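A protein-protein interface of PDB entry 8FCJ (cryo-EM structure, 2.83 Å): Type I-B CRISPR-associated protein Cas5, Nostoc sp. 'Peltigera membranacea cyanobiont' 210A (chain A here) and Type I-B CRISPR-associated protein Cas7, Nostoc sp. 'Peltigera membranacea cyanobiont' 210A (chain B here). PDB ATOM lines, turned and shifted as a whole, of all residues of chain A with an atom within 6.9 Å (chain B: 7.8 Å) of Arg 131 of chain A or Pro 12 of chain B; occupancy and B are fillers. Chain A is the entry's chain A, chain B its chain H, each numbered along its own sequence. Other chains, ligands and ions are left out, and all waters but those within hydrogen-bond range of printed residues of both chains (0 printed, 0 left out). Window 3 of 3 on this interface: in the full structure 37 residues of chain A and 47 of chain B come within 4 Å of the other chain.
Of the 13 printed residues of chain A, 6 touch a printed residue of chain B.
Hydrophobic or aromatic side chains of chain A that line the printed part of chain B: Leu 43.
Among the printed residues, 8 pairs touch across the chains.
N of Tyr 15 of chain B lies within hydrogen-bond range of O of Thr 231 of chain B (2.8 Å).
O of Ser 42 of chain A sits at hydrogen-bond distance from NE of Arg 132 of chain A, 2.8 Å away.
OG1 of Thr 189 of chain B is in hydrogen-bond range of O of Pro 12 of chain B (3.5 Å).
The backbone carbonyl oxygen of Glu 128 of chain A sits at hydrogen-bond distance from the guanidinium group of Arg 131 of chain A.
OH of Tyr 15 of chain B sits at hydrogen-bond distance from ND2 of Asn 13 of chain B, at 2.6 Å.
The guanidinium group (NH1) of Arg 131 of chain A lies close to the backbone carbonyl oxygen (O) of Leu 129 of chain A, at 3.5 Å.
The guanidinium group (NH1) of Arg 132 of chain A lies within hydrogen-bond range of the side-chain hydroxyl (OH) of Tyr 15 of chain B, at 3.0 Å.
OD1 of Asn 13 of chain B lies close to O of Arg 132 of chain A, at 3.1 Å.
Leu 43 of chain A touches Phe 234 of chain B (CD1 to CE1, 3.4 Å).
O of Asn 232 of chain B touches O of Pro 127 of chain A (3.9 Å).
Glu 128 of chain A touches Asn 232 of chain B (CB to ND2, 3.5 Å).
Pro 12 of chain B touches Arg 131 of chain A (N to CZ, 3.7 Å).
Arg 132 of chain A touches Asp 187 of chain B (O to OD2, 3.7 Å).
Phe 133 of chain A touches Asp 187 of chain B.
Of chain B, only Pro 12 comes within 4 Å of Arg 131 of chain A.
Of chain A, only Arg 131 comes within 4 Å of Pro 12 of chain B.
Of the printed residues of chain B, Leu 43 of chain A touches Phe 234.
Of the printed residues of chain A, Asn 232 of chain B touches Pro 127 (3.9 Å) and Glu 128 (3.5 Å).
Printed residues of chain B within 4 Å of Pro 127 of chain A: Asn 232.
Printed residues of chain B within 4 Å of Arg 132 of chain A: Asn 13, Tyr 15 and Asp 187.
Of the printed residues of chain A, Tyr 15 of chain B touches Arg 132 (3.0 Å).
Phe 194 of chain B touches none of the printed residues of chain A.
The nearest printed residue of chain B that does not touch Arg 132 of chain A is Phe 234 of chain B (4.2 Å).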
ATOM      1  N   SER A  42      18.348 -12.081   2.750  1.00  0.00           N
ATOM      2  CA  SER A  42      19.347 -13.143   2.764  1.00  0.00           C
ATOM      3  C   SER A  42      20.746 -12.584   2.547  1.00  0.00           C
ATOM      4  O   SER A  42      21.714 -13.053   3.155  1.00  0.00           O
ATOM      5  CB  SER A  42      19.018 -14.186   1.698  1.00  0.00           C
ATOM      6  OG  SER A  42      20.126 -15.034   1.458  1.00  0.00           O
ATOM      7  N   LEU A  43      20.869 -11.587   1.671  1.00  0.00           N
ATOM      8  CA  LEU A  43      22.168 -10.989   1.388  1.00  0.00           C
ATOM      9  C   LEU A  43      22.757 -10.337   2.630  1.00  0.00           C
ATOM     10  O   LEU A  43      23.952 -10.484   2.909  1.00  0.00           O
ATOM     11  CB  LEU A  43      22.031  -9.972   0.257  1.00  0.00           C
ATOM     12  CG  LEU A  43      23.161  -8.964   0.065  1.00  0.00           C
ATOM     13  CD1 LEU A  43      24.443  -9.678  -0.286  1.00  0.00           C
ATOM     14  CD2 LEU A  43      22.795  -7.968  -1.016  1.00  0.00           C
ATOM     15  N   VAL A  44      21.933  -9.613   3.395  1.00  0.00           N
ATOM     16  CA  VAL A  44      22.407  -9.006   4.634  1.00  0.00           C
ATOM     17  C   VAL A  44      22.312  -9.954   5.818  1.00  0.00           C
ATOM     18  O   VAL A  44      22.669  -9.568   6.940  1.00  0.00           O
ATOM     19  CB  VAL A  44      21.639  -7.707   4.949  1.00  0.00           C
ATOM     20  CG1 VAL A  44      21.810  -6.714   3.822  1.00  0.00           C
ATOM     21  CG2 VAL A  44      20.171  -8.004   5.182  1.00  0.00           C
ATOM     22  N   GLY A  45      21.852 -11.182   5.607  1.00  0.00           N
ATOM     23  CA  GLY A  45      21.750 -12.151   6.685  1.00  0.00           C
ATOM     24  C   GLY A  45      20.731 -11.807   7.748  1.00  0.00           C
ATOM     25  O   GLY A  45      21.000 -11.993   8.941  1.00  0.00           O
ATOM     26  N   GLU A  46      19.562 -11.316   7.348  1.00  0.00           N
ATOM     27  CA  GLU A  46      18.504 -10.934   8.276  1.00  0.00           C
ATOM     28  C   GLU A  46      17.396 -11.976   8.203  1.00  0.00           C
ATOM     29  O   GLU A  46      16.689 -12.068   7.194  1.00  0.00           O
ATOM     30  CB  GLU A  46      17.968  -9.543   7.950  1.00  0.00           C
ATOM     31  CG  GLU A  46      16.904  -9.062   8.912  1.00  0.00           C
ATOM     32  CD  GLU A  46      17.335  -9.194  10.356  1.00  0.00           C
ATOM     33  OE1 GLU A  46      18.377  -8.609  10.721  1.00  0.00           O
ATOM     34  OE2 GLU A  46      16.638  -9.884  11.127  1.00  0.00           O
ATOM     35  N   ARG A 119      22.738  -1.465   5.325  1.00  0.00           N
ATOM     36  CA  ARG A 119      23.233  -2.818   5.556  1.00  0.00           C
ATOM     37  C   ARG A 119      23.801  -3.427   4.281  1.00  0.00           C
ATOM     38  O   ARG A 119      24.849  -4.080   4.316  1.00  0.00           O
ATOM     39  CB  ARG A 119      22.119  -3.695   6.124  1.00  0.00           C
ATOM     40  CG  ARG A 119      21.760  -3.371   7.558  1.00  0.00           C
ATOM     41  CD  ARG A 119      20.775  -4.377   8.119  1.00  0.00           C
ATOM     42  NE  ARG A 119      21.426  -5.620   8.510  1.00  0.00           N
ATOM     43  CZ  ARG A 119      20.794  -6.664   9.027  1.00  0.00           C
ATOM     44  NH1 ARG A 119      19.487  -6.653   9.223  1.00  0.00           N
ATOM     45  NH2 ARG A 119      21.492  -7.748   9.352  1.00  0.00           N
ATOM     46  N   PRO A 127      32.856  -7.511   2.832  1.00  0.00           N
ATOM     47  CA  PRO A 127      32.183  -8.814   2.727  1.00  0.00           C
ATOM     48  C   PRO A 127      32.610  -9.812   3.788  1.00  0.00           C
ATOM     49  O   PRO A 127      31.870 -10.767   4.047  1.00  0.00           O
ATOM     50  CB  PRO A 127      32.565  -9.295   1.321  1.00  0.00           C
ATOM     51  CG  PRO A 127      33.801  -8.538   0.982  1.00  0.00           C
ATOM     52  CD  PRO A 127      33.656  -7.202   1.637  1.00  0.00           C
ATOM     53  N   GLU A 128      33.774  -9.629   4.408  1.00  0.00           N
ATOM     54  CA  GLU A 128      34.232 -10.552   5.437  1.00  0.00           C
ATOM     55  C   GLU A 128      33.516 -10.364   6.767  1.00  0.00           C
ATOM     56  O   GLU A 128      33.668 -11.209   7.655  1.00  0.00           O
ATOM     57  CB  GLU A 128      35.740 -10.406   5.643  1.00  0.00           C
ATOM     58  CG  GLU A 128      36.150  -9.111   6.318  1.00  0.00           C
ATOM     59  CD  GLU A 128      36.447  -8.009   5.325  1.00  0.00           C
ATOM     60  OE1 GLU A 128      36.542  -8.306   4.116  1.00  0.00           O
ATOM     61  OE2 GLU A 128      36.589  -6.844   5.752  1.00  0.00           O
ATOM     62  N   LEU A 129      32.748  -9.289   6.930  1.00  0.00           N
ATOM     63  CA  LEU A 129      32.021  -9.027   8.164  1.00  0.00           C
ATOM     64  C   LEU A 129      30.548  -9.403   8.072  1.00  0.00           C
ATOM     65  O   LEU A 129      29.787  -9.113   8.999  1.00  0.00           O
ATOM     66  CB  LEU A 129      32.157  -7.557   8.554  1.00  0.00           C
ATOM     67  CG  LEU A 129      33.576  -7.056   8.819  1.00  0.00           C
ATOM     68  CD1 LEU A 129      33.557  -5.582   9.177  1.00  0.00           C
ATOM     69  CD2 LEU A 129      34.225  -7.868   9.923  1.00  0.00           C
ATOM     70  N   VAL A 130      30.130 -10.037   6.983  1.00  0.00           N
ATOM     71  CA  VAL A 130      28.738 -10.425   6.796  1.00  0.00           C
ATOM     72  C   VAL A 130      28.522 -11.797   7.417  1.00  0.00           C
ATOM     73  O   VAL A 130      29.254 -12.747   7.119  1.00  0.00           O
ATOM     74  CB  VAL A 130      28.366 -10.433   5.305  1.00  0.00           C
ATOM     75  CG1 VAL A 130      26.860 -10.452   5.139  1.00  0.00           C
ATOM     76  CG2 VAL A 130      28.965  -9.228   4.609  1.00  0.00           C
ATOM     77  N   ARG A 131      27.520 -11.900   8.282  1.00  0.00           N
ATOM     78  CA  ARG A 131      27.174 -13.150   8.954  1.00  0.00           C
ATOM     79  C   ARG A 131      25.864 -13.652   8.359  1.00  0.00           C
ATOM     80  O   ARG A 131      24.790 -13.126   8.665  1.00  0.00           O
ATOM     81  CB  ARG A 131      27.068 -12.945  10.460  1.00  0.00           C
ATOM     82  CG  ARG A 131      28.376 -12.545  11.117  1.00  0.00           C
ATOM     83  CD  ARG A 131      29.370 -13.693  11.107  1.00  0.00           C
ATOM     84  NE  ARG A 131      30.703 -13.271  11.524  1.00  0.00           N
ATOM     85  CZ  ARG A 131      31.546 -12.590  10.763  1.00  0.00           C
ATOM     86  NH1 ARG A 131      31.236 -12.244   9.525  1.00  0.00           N
ATOM     87  NH2 ARG A 131      32.734 -12.248  11.255  1.00  0.00           N
ATOM     88  N   ARG A 132      25.957 -14.672   7.510  1.00  0.00           N
ATOM     89  CA  ARG A 132      24.804 -15.223   6.818  1.00  0.00           C
ATOM     90  C   ARG A 132      25.044 -16.703   6.560  1.00  0.00           C
ATOM     91  O   ARG A 132      26.166 -17.200   6.680  1.00  0.00           O
ATOM     92  CB  ARG A 132      24.533 -14.477   5.509  1.00  0.00           C
ATOM     93  CG  ARG A 132      25.763 -14.280   4.647  1.00  0.00           C
ATOM     94  CD  ARG A 132      25.395 -13.722   3.290  1.00  0.00           C
ATOM     95  NE  ARG A 132      24.166 -14.313   2.779  1.00  0.00           N
ATOM     96  CZ  ARG A 132      24.118 -15.393   2.013  1.00  0.00           C
ATOM     97  NH1 ARG A 132      25.219 -16.029   1.649  1.00  0.00           N
ATOM     98  NH2 ARG A 132      22.938 -15.847   1.606  1.00  0.00           N
ATOM     99  N   PHE A 133      23.977 -17.412   6.204  1.00  0.00           N
ATOM    100  CA  PHE A 133      24.045 -18.844   5.965  1.00  0.00           C
ATOM    101  C   PHE A 133      23.482 -19.174   4.592  1.00  0.00           C
ATOM    102  O   PHE A 133      22.565 -18.513   4.103  1.00  0.00           O
ATOM    103  CB  PHE A 133      23.288 -19.631   7.045  1.00  0.00           C
ATOM    104  CG  PHE A 133      21.814 -19.349   7.082  1.00  0.00           C
ATOM    105  CD1 PHE A 133      21.315 -18.318   7.856  1.00  0.00           C
ATOM    106  CD2 PHE A 133      20.926 -20.124   6.358  1.00  0.00           C
ATOM    107  CE1 PHE A 133      19.962 -18.059   7.897  1.00  0.00           C
ATOM    108  CE2 PHE A 133      19.573 -19.867   6.395  1.00  0.00           C
ATOM    109  CZ  PHE A 133      19.091 -18.835   7.167  1.00  0.00           C
ATOM    110  N   PRO B  12      33.248 -15.874  10.162  1.00  0.00           N
ATOM    111  CA  PRO B  12      33.617 -15.599   8.770  1.00  0.00           C
ATOM    112  C   PRO B  12      33.123 -16.685   7.826  1.00  0.00           C
ATOM    113  O   PRO B  12      33.591 -17.818   7.903  1.00  0.00           O
ATOM    114  CB  PRO B  12      35.152 -15.569   8.805  1.00  0.00           C
ATOM    115  CG  PRO B  12      35.530 -15.593  10.261  1.00  0.00           C
ATOM    116  CD  PRO B  12      34.412 -16.276  10.963  1.00  0.00           C
ATOM    117  N   ASN B  13      32.186 -16.339   6.950  1.00  0.00           N
ATOM    118  CA  ASN B  13      31.647 -17.309   6.011  1.00  0.00           C
ATOM    119  C   ASN B  13      32.713 -17.748   5.017  1.00  0.00           C
ATOM    120  O   ASN B  13      33.620 -16.990   4.668  1.00  0.00           O
ATOM    121  CB  ASN B  13      30.452 -16.724   5.264  1.00  0.00           C
ATOM    122  CG  ASN B  13      29.161 -16.867   6.033  1.00  0.00           C
ATOM    123  OD1 ASN B  13      29.165 -17.005   7.254  1.00  0.00           O
ATOM    124  ND2 ASN B  13      28.044 -16.839   5.320  1.00  0.00           N
ATOM    125  N   TYR B  14      32.602 -18.995   4.569  1.00  0.00           N
ATOM    126  CA  TYR B  14      33.501 -19.543   3.561  1.00  0.00           C
ATOM    127  C   TYR B  14      32.666 -20.297   2.542  1.00  0.00           C
ATOM    128  O   TYR B  14      32.047 -21.311   2.877  1.00  0.00           O
ATOM    129  CB  TYR B  14      34.549 -20.463   4.189  1.00  0.00           C
ATOM    130  CG  TYR B  14      35.816 -19.750   4.590  1.00  0.00           C
ATOM    131  CD1 TYR B  14      36.627 -19.152   3.639  1.00  0.00           C
ATOM    132  CD2 TYR B  14      36.199 -19.671   5.919  1.00  0.00           C
ATOM    133  CE1 TYR B  14      37.783 -18.498   4.000  1.00  0.00           C
ATOM    134  CE2 TYR B  14      37.354 -19.019   6.289  1.00  0.00           C
ATOM    135  CZ  TYR B  14      38.142 -18.434   5.326  1.00  0.00           C
ATOM    136  OH  TYR B  14      39.295 -17.782   5.691  1.00  0.00           O
ATOM    137  N   TYR B  15      32.648 -19.806   1.310  1.00  0.00           N
ATOM    138  CA  TYR B  15      31.876 -20.410   0.237  1.00  0.00           C
ATOM    139  C   TYR B  15      32.814 -21.033  -0.786  1.00  0.00           C
ATOM    140  O   TYR B  15      33.898 -20.505  -1.050  1.00  0.00           O
ATOM    141  CB  TYR B  15      30.987 -19.383  -0.466  1.00  0.00           C
ATOM    142  CG  TYR B  15      30.194 -18.474   0.438  1.00  0.00           C
ATOM    143  CD1 TYR B  15      30.745 -17.301   0.929  1.00  0.00           C
ATOM    144  CD2 TYR B  15      28.883 -18.771   0.774  1.00  0.00           C
ATOM    145  CE1 TYR B  15      30.022 -16.461   1.743  1.00  0.00           C
ATOM    146  CE2 TYR B  15      28.151 -17.935   1.588  1.00  0.00           C
ATOM    147  CZ  TYR B  15      28.725 -16.783   2.070  1.00  0.00           C
ATOM    148  OH  TYR B  15      28.000 -15.946   2.883  1.00  0.00           O
ATOM    149  N   ASP B 187      27.840 -23.188   1.071  1.00  0.00           N
ATOM    150  CA  ASP B 187      28.246 -22.410   2.237  1.00  0.00           C
ATOM    151  C   ASP B 187      28.874 -23.383   3.224  1.00  0.00           C
ATOM    152  O   ASP B 187      28.177 -24.012   4.022  1.00  0.00           O
ATOM    153  CB  ASP B 187      27.058 -21.678   2.846  1.00  0.00           C
ATOM    154  CG  ASP B 187      27.460 -20.776   3.988  1.00  0.00           C
ATOM    155  OD1 ASP B 187      28.661 -20.464   4.107  1.00  0.00           O
ATOM    156  OD2 ASP B 187      26.577 -20.378   4.772  1.00  0.00           O
ATOM    157  N   ALA B 188      30.202 -23.516   3.162  1.00  0.00           N
ATOM    158  CA  ALA B 188      30.891 -24.487   4.005  1.00  0.00           C
ATOM    159  C   ALA B 188      30.682 -24.201   5.485  1.00  0.00           C
ATOM    160  O   ALA B 188      30.683 -25.128   6.301  1.00  0.00           O
ATOM    161  CB  ALA B 188      32.381 -24.503   3.675  1.00  0.00           C
ATOM    162  N   THR B 189      30.505 -22.931   5.849  1.00  0.00           N
ATOM    163  CA  THR B 189      30.250 -22.589   7.242  1.00  0.00           C
ATOM    164  C   THR B 189      28.880 -23.090   7.688  1.00  0.00           C
ATOM    165  O   THR B 189      28.701 -23.478   8.848  1.00  0.00           O
ATOM    166  CB  THR B 189      30.377 -21.077   7.429  1.00  0.00           C
ATOM    167  OG1 THR B 189      31.759 -20.708   7.361  1.00  0.00           O
ATOM    168  CG2 THR B 189      29.816 -20.638   8.771  1.00  0.00           C
ATOM    169  N   PHE B 194      31.942 -29.431   9.645  1.00  0.00           N
ATOM    170  CA  PHE B 194      32.726 -28.760   8.612  1.00  0.00           C
ATOM    171  C   PHE B 194      33.484 -29.749   7.737  1.00  0.00           C
ATOM    172  O   PHE B 194      33.773 -29.447   6.575  1.00  0.00           O
ATOM    173  CB  PHE B 194      33.696 -27.770   9.255  1.00  0.00           C
ATOM    174  CG  PHE B 194      33.065 -26.465   9.649  1.00  0.00           C
ATOM    175  CD1 PHE B 194      31.849 -26.432  10.307  1.00  0.00           C
ATOM    176  CD2 PHE B 194      33.704 -25.269   9.384  1.00  0.00           C
ATOM    177  CE1 PHE B 194      31.275 -25.235  10.672  1.00  0.00           C
ATOM    178  CE2 PHE B 194      33.135 -24.069   9.750  1.00  0.00           C
ATOM    179  CZ  PHE B 194      31.919 -24.053  10.394  1.00  0.00           C
ATOM    180  N   THR B 231      36.315 -18.663  -1.461  1.00  0.00           N
ATOM    181  CA  THR B 231      36.335 -17.273  -1.037  1.00  0.00           C
ATOM    182  C   THR B 231      35.325 -17.066   0.080  1.00  0.00           C
ATOM    183  O   THR B 231      34.429 -17.884   0.296  1.00  0.00           O
ATOM    184  CB  THR B 231      36.024 -16.326  -2.198  1.00  0.00           C
ATOM    185  OG1 THR B 231      35.937 -14.983  -1.708  1.00  0.00           O
ATOM    186  CG2 THR B 231      34.705 -16.704  -2.842  1.00  0.00           C
ATOM    187  N   ASN B 232      35.489 -15.955   0.791  1.00  0.00           N
ATOM    188  CA  ASN B 232      34.548 -15.535   1.819  1.00  0.00           C
ATOM    189  C   ASN B 232      33.508 -14.554   1.297  1.00  0.00           C
ATOM    190  O   ASN B 232      32.700 -14.052   2.082  1.00  0.00           O
ATOM    191  CB  ASN B 232      35.298 -14.910   2.997  1.00  0.00           C
ATOM    192  CG  ASN B 232      36.393 -13.970   2.552  1.00  0.00           C
ATOM    193  OD1 ASN B 232      37.015 -14.173   1.511  1.00  0.00           O
ATOM    194  ND2 ASN B 232      36.637 -12.931   3.340  1.00  0.00           N
ATOM    195  N   PHE B 234      30.123 -13.432  -0.651  1.00  0.00           N
ATOM    196  CA  PHE B 234      28.822 -14.046  -0.884  1.00  0.00           C
ATOM    197  C   PHE B 234      28.486 -14.186  -2.362  1.00  0.00           C
ATOM    198  O   PHE B 234      27.495 -14.844  -2.690  1.00  0.00           O
ATOM    199  CB  PHE B 234      27.729 -13.237  -0.186  1.00  0.00           C
ATOM    200  CG  PHE B 234      27.852 -11.757  -0.383  1.00  0.00           C
ATOM    201  CD1 PHE B 234      27.440 -11.165  -1.562  1.00  0.00           C
ATOM    202  CD2 PHE B 234      28.381 -10.957   0.610  1.00  0.00           C
ATOM    203  CE1 PHE B 234      27.558  -9.807  -1.747  1.00  0.00           C
ATOM    204  CE2 PHE B 234      28.498  -9.597   0.431  1.00  0.00           C
ATOM    205  CZ  PHE B 234      28.084  -9.022  -0.748  1.00  0.00           C
ATOM    206  N   ASP B 316      41.803 -23.401   6.268  1.00  0.00           N
ATOM    207  CA  ASP B 316      40.925 -22.267   6.540  1.00  0.00           C
ATOM    208  C   ASP B 316      39.815 -22.633   7.516  1.00  0.00           C
ATOM    209  O   ASP B 316      39.454 -21.830   8.383  1.00  0.00           O
ATOM    210  CB  ASP B 316      40.335 -21.740   5.235  1.00  0.00           C
ATOM    211  CG  ASP B 316      41.295 -20.842   4.485  1.00  0.00           C
ATOM    212  OD1 ASP B 316      42.461 -20.728   4.914  1.00  0.00           O
ATOM    213  OD2 ASP B 316      40.885 -20.251   3.465  1.00  0.00           O
ATOM    214  N   LEU B 317      39.257 -23.833   7.391  1.00  0.00           N
ATOM    215  CA  LEU B 317      38.137 -24.261   8.218  1.00  0.00           C
ATOM    216  C   LEU B 317      38.572 -24.888   9.535  1.00  0.00           C
ATOM    217  O   LEU B 317      37.711 -25.241  10.347  1.00  0.00           O
ATOM    218  CB  LEU B 317      37.263 -25.252   7.447  1.00  0.00           C
ATOM    219  CG  LEU B 317      36.444 -24.684   6.288  1.00  0.00           C
ATOM    220  CD1 LEU B 317      35.584 -25.764   5.663  1.00  0.00           C
ATOM    221  CD2 LEU B 317      35.589 -23.527   6.760  1.00  0.00           C
